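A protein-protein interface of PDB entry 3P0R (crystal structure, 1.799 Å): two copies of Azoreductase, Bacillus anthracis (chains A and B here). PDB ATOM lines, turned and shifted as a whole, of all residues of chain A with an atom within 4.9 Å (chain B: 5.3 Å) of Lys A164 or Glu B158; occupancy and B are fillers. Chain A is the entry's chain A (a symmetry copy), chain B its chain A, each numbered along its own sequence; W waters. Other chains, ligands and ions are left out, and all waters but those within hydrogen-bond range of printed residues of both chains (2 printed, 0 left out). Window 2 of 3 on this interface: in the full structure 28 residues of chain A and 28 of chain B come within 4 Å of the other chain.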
ATOM      1  N   GLU A 160      14.656   0.163 -18.200  1.00  0.00           N
ATOM      2  CA  GLU A 160      15.517  -0.553 -17.246  1.00  0.00           C
ATOM      3  C   GLU A 160      16.257  -1.615 -18.032  1.00  0.00           C
ATOM      4  O   GLU A 160      15.635  -2.539 -18.575  1.00  0.00           O
ATOM      5  CB  GLU A 160      14.687  -1.200 -16.149  1.00  0.00           C
ATOM      6  CG  GLU A 160      15.478  -1.500 -14.865  1.00  0.00           C
ATOM      7  CD  GLU A 160      16.500  -2.620 -15.019  1.00  0.00           C
ATOM      8  OE1 GLU A 160      16.153  -3.690 -15.554  1.00  0.00           O
ATOM      9  OE2 GLU A 160      17.653  -2.457 -14.571  1.00  0.00           O
ATOM     10  N   MET A 161      17.572  -1.453 -18.160  1.00  0.00           N
ATOM     11  CA  MET A 161      18.375  -2.402 -18.927  1.00  0.00           C
ATOM     12  C   MET A 161      19.591  -2.927 -18.165  1.00  0.00           C
ATOM     13  O   MET A 161      20.629  -3.295 -18.757  1.00  0.00           O
ATOM     14  CB  MET A 161      18.768  -1.775 -20.275  1.00  0.00           C
ATOM     15  CG  MET A 161      17.558  -1.651 -21.200  1.00  0.00           C
ATOM     16  SD  MET A 161      17.910  -0.797 -22.902  1.00  0.00           S
ATOM     17  CE  MET A 161      17.649   1.075 -22.376  1.00  0.00           C
ATOM     18  N   ALA A 162      19.505  -2.911 -16.840  1.00  0.00           N
ATOM     19  CA  ALA A 162      20.578  -3.387 -16.002  1.00  0.00           C
ATOM     20  C   ALA A 162      20.222  -4.798 -15.444  1.00  0.00           C
ATOM     21  O   ALA A 162      20.729  -5.809 -15.941  1.00  0.00           O
ATOM     22  CB  ALA A 162      20.870  -2.397 -14.909  1.00  0.00           C
ATOM     23  N   VAL A 163      19.274  -4.856 -14.518  1.00  0.00           N
ATOM     24  CA  VAL A 163      18.709  -6.142 -14.044  1.00  0.00           C
ATOM     25  C   VAL A 163      18.164  -6.962 -15.189  1.00  0.00           C
ATOM     26  O   VAL A 163      18.441  -8.185 -15.318  1.00  0.00           O
ATOM     27  CB  VAL A 163      17.606  -5.912 -12.991  1.00  0.00           C
ATOM     28  CG1 VAL A 163      16.937  -7.228 -12.631  1.00  0.00           C
ATOM     29  CG2 VAL A 163      18.197  -5.241 -11.733  1.00  0.00           C
ATOM     30  N   LYS A 164      17.352  -6.311 -16.018  1.00  0.00           N
ATOM     31  CA  LYS A 164      16.780  -6.977 -17.196  1.00  0.00           C
ATOM     32  C   LYS A 164      17.857  -7.593 -18.109  1.00  0.00           C
ATOM     33  O   LYS A 164      17.679  -8.726 -18.615  1.00  0.00           O
ATOM     34  CB  LYS A 164      15.897  -6.023 -17.972  1.00  0.00           C
ATOM     35  CG  LYS A 164      15.237  -6.664 -19.172  1.00  0.00           C
ATOM     36  CD  LYS A 164      14.264  -5.638 -19.836  1.00  0.00           C
ATOM     37  CE  LYS A 164      13.621  -6.197 -21.069  1.00  0.00           C
ATOM     38  NZ  LYS A 164      12.678  -5.213 -21.696  1.00  0.00           N
ATOM     39  N   TYR A 165      18.981  -6.902 -18.277  1.00  0.00           N
ATOM     40  CA  TYR A 165      20.065  -7.424 -19.078  1.00  0.00           C
ATOM     41  C   TYR A 165      20.638  -8.706 -18.461  1.00  0.00           C
ATOM     42  O   TYR A 165      20.705  -9.790 -19.098  1.00  0.00           O
ATOM     43  CB  TYR A 165      21.194  -6.375 -19.316  1.00  0.00           C
ATOM     44  CG  TYR A 165      22.190  -6.997 -20.272  1.00  0.00           C
ATOM     45  CD1 TYR A 165      21.897  -7.076 -21.618  1.00  0.00           C
ATOM     46  CD2 TYR A 165      23.383  -7.590 -19.818  1.00  0.00           C
ATOM     47  CE1 TYR A 165      22.748  -7.686 -22.505  1.00  0.00           C
ATOM     48  CE2 TYR A 165      24.253  -8.224 -20.694  1.00  0.00           C
ATOM     49  CZ  TYR A 165      23.938  -8.263 -22.062  1.00  0.00           C
ATOM     50  OH  TYR A 165      24.761  -8.909 -22.961  1.00  0.00           O
ATOM     51  N   VAL A 166      21.016  -8.596 -17.217  1.00  0.00           N
ATOM     52  CA  VAL A 166      21.675  -9.727 -16.556  1.00  0.00           C
ATOM     53  C   VAL A 166      20.726 -10.926 -16.460  1.00  0.00           C
ATOM     54  O   VAL A 166      21.132 -12.069 -16.752  1.00  0.00           O
ATOM     55  CB  VAL A 166      22.246  -9.419 -15.180  1.00  0.00           C
ATOM     56  CG1 VAL A 166      23.045 -10.598 -14.725  1.00  0.00           C
ATOM     57  CG2 VAL A 166      23.194  -8.146 -15.193  1.00  0.00           C
ATOM     58  N   ALA A 167      19.483 -10.657 -16.063  1.00  0.00           N
ATOM     59  CA  ALA A 167      18.449 -11.695 -15.954  1.00  0.00           C
ATOM     60  C   ALA A 167      18.216 -12.397 -17.277  1.00  0.00           C
ATOM     61  O   ALA A 167      18.076 -13.598 -17.335  1.00  0.00           O
ATOM     62  CB  ALA A 167      17.176 -11.117 -15.375  1.00  0.00           C
ATOM     63  N   SER A 168      18.187 -11.638 -18.355  1.00  0.00           N
ATOM     64  CA  SER A 168      17.951 -12.196 -19.673  1.00  0.00           C
ATOM     65  C   SER A 168      19.039 -13.138 -20.138  1.00  0.00           C
ATOM     66  O   SER A 168      18.752 -14.215 -20.682  1.00  0.00           O
ATOM     67  CB  SER A 168      17.770 -11.067 -20.674  1.00  0.00           C
ATOM     68  OG  SER A 168      16.537 -10.410 -20.441  1.00  0.00           O
ATOM     69  N   GLY B 154       7.776 -11.229 -32.250  1.00  0.00           N
ATOM     70  CA  GLY B 154       8.125 -12.568 -31.784  1.00  0.00           C
ATOM     71  C   GLY B 154       8.748 -12.651 -30.390  1.00  0.00           C
ATOM     72  O   GLY B 154       8.804 -11.687 -29.655  1.00  0.00           O
ATOM     73  N   PRO B 155       9.230 -13.840 -30.022  1.00  0.00           N
ATOM     74  CA  PRO B 155       9.719 -14.045 -28.660  1.00  0.00           C
ATOM     75  C   PRO B 155      10.911 -13.171 -28.232  1.00  0.00           C
ATOM     76  O   PRO B 155      11.111 -12.982 -27.025  1.00  0.00           O
ATOM     77  CB  PRO B 155      10.085 -15.550 -28.654  1.00  0.00           C
ATOM     78  CG  PRO B 155       9.306 -16.143 -29.710  1.00  0.00           C
ATOM     79  CD  PRO B 155       9.132 -15.109 -30.773  1.00  0.00           C
ATOM     80  N   ALA B 156      11.697 -12.634 -29.187  1.00  0.00           N
ATOM     81  CA  ALA B 156      12.844 -11.799 -28.835  1.00  0.00           C
ATOM     82  C   ALA B 156      12.507 -10.306 -28.743  1.00  0.00           C
ATOM     83  O   ALA B 156      13.372  -9.514 -28.423  1.00  0.00           O
ATOM     84  CB  ALA B 156      14.005 -12.009 -29.838  1.00  0.00           C
ATOM     85  N   ALA B 157      11.270  -9.924 -29.030  1.00  0.00           N
ATOM     86  CA  ALA B 157      10.934  -8.511 -29.180  1.00  0.00           C
ATOM     87  C   ALA B 157      11.157  -7.776 -27.867  1.00  0.00           C
ATOM     88  O   ALA B 157      11.571  -6.627 -27.897  1.00  0.00           O
ATOM     89  CB  ALA B 157       9.497  -8.312 -29.629  1.00  0.00           C
ATOM     90  N   GLU B 158      10.915  -8.421 -26.726  1.00  0.00           N
ATOM     91  CA  GLU B 158      11.052  -7.692 -25.431  1.00  0.00           C
ATOM     92  C   GLU B 158      12.494  -7.581 -24.939  1.00  0.00           C
ATOM     93  O   GLU B 158      12.740  -6.865 -23.955  1.00  0.00           O
ATOM     94  CB  GLU B 158      10.166  -8.264 -24.290  1.00  0.00           C
ATOM     95  CG  GLU B 158       8.630  -8.086 -24.451  1.00  0.00           C
ATOM     96  CD  GLU B 158       8.192  -6.740 -25.083  1.00  0.00           C
ATOM     97  OE1 GLU B 158       8.587  -5.652 -24.598  1.00  0.00           O
ATOM     98  OE2 GLU B 158       7.431  -6.780 -26.084  1.00  0.00           O
ATOM     99  N   VAL B 159      13.441  -8.270 -25.590  1.00  0.00           N
ATOM    100  CA  VAL B 159      14.843  -8.231 -25.144  1.00  0.00           C
ATOM    101  C   VAL B 159      15.815  -7.543 -26.123  1.00  0.00           C
ATOM    102  O   VAL B 159      17.024  -7.738 -26.042  1.00  0.00           O
ATOM    103  CB  VAL B 159      15.351  -9.644 -24.731  1.00  0.00           C
ATOM    104  CG1 VAL B 159      14.566 -10.169 -23.501  1.00  0.00           C
ATOM    105  CG2 VAL B 159      15.315 -10.642 -25.896  1.00  0.00           C
ATOM    106  N   GLU B 160      15.303  -6.705 -27.016  1.00  0.00           N
ATOM    107  CA  GLU B 160      16.175  -5.916 -27.898  1.00  0.00           C
ATOM    108  C   GLU B 160      16.759  -4.799 -27.059  1.00  0.00           C
ATOM    109  O   GLU B 160      16.019  -3.932 -26.571  1.00  0.00           O
ATOM    110  CB  GLU B 160      15.386  -5.337 -29.062  1.00  0.00           C
ATOM    111  CG  GLU B 160      16.252  -4.968 -30.279  1.00  0.00           C
ATOM    112  CD  GLU B 160      17.161  -3.767 -30.045  1.00  0.00           C
ATOM    113  OE1 GLU B 160      16.683  -2.732 -29.544  1.00  0.00           O
ATOM    114  OE2 GLU B 160      18.356  -3.832 -30.398  1.00  0.00           O
ATOM    115  N   MET B 161      18.067  -4.852 -26.823  1.00  0.00           N
ATOM    116  CA  MET B 161      18.724  -3.842 -25.997  1.00  0.00           C
ATOM    117  C   MET B 161      19.950  -3.214 -26.660  1.00  0.00           C
ATOM    118  O   MET B 161      20.902  -2.763 -25.987  1.00  0.00           O
ATOM    119  CB  MET B 161      19.056  -4.438 -24.620  1.00  0.00           C
ATOM    120  CG  MET B 161      17.790  -4.666 -23.795  1.00  0.00           C
ATOM    121  SD  MET B 161      18.073  -5.493 -22.067  1.00  0.00           S
ATOM    122  CE  MET B 161      18.012  -7.378 -22.607  1.00  0.00           C
ATOM    123  N   LYS B 164      17.618  -0.021 -28.993  1.00  0.00           N
ATOM    124  CA  LYS B 164      16.899   0.590 -27.868  1.00  0.00           C
ATOM    125  C   LYS B 164      17.843   1.291 -26.872  1.00  0.00           C
ATOM    126  O   LYS B 164      17.531   2.404 -26.387  1.00  0.00           O
ATOM    127  CB  LYS B 164      16.039  -0.436 -27.163  1.00  0.00           C
ATOM    128  CG  LYS B 164      15.232   0.143 -26.023  1.00  0.00           C
ATOM    129  CD  LYS B 164      14.297  -0.962 -25.437  1.00  0.00           C
ATOM    130  CE  LYS B 164      13.511  -0.463 -24.262  1.00  0.00           C
ATOM    131  NZ  LYS B 164      12.606  -1.524 -23.710  1.00  0.00           N
HETATM  132  O   HOH W   1      13.838  -4.166 -24.505  1.00  0.00           O
HETATM  133  O   HOH W   2      13.617  -2.481 -20.813  1.00  0.00           O
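Water W1 lies within hydrogen-bond range of O of Glu B158 (3.0 Å), O of Glu B160 (3.0 Å), NZ of Lys B164 (3.0 Å) and NZ of Lys A164 (3.2 Å). Water W2 lies within hydrogen-bond range of O of Glu A160 (3.0 Å), NZ of Lys A164 (3.0 Å) and NZ of Lys B164 (3.2 Å).
Met A161 touches Met B161. OG of Ser A168 touches CG1 of Val B159, 3.6 Å away.
Met A161 touches its own counterpart, Met B161. Positions printed for both chains: 160, 161 and 164.
Hydrophobic or aromatic side chains of chain A that line the printed part of chain B: Met A161. Among the printed residues, no Asp or Glu carboxylate lies within 4 Å of a Lys or Arg side-chain nitrogen of the other chain.
Of the printed residues of chain B, Met A161 touches Met B161 (3.97 Å). Ala A162 touches none of the printed residues of chain B. Of chain B, only Glu B158 comes within 4 Å of Lys A164. Printed residues of chain B within 4 Å of Ser A168: Val B159. Of the printed residues of chain A, Glu B158 touches Lys A164. Of the printed residues of chain A, Val B159 touches Ser A168. Of the printed residues of chain A, Met B161 touches Met A161. The nearest printed residue of chain A that does not touch Glu B158 is Ser A168 (6.3 Å).
O of Glu B158 sits at hydrogen-bond distance from NZ of Lys A164 (2.8 Å).
The side-chain carboxylate (OE1) of Glu A160 lies within hydrogen-bond range of the backbone NH (N) of Lys A164 (2.9 Å). OG of Ser A168 sits at hydrogen-bond distance from O of Lys A164.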
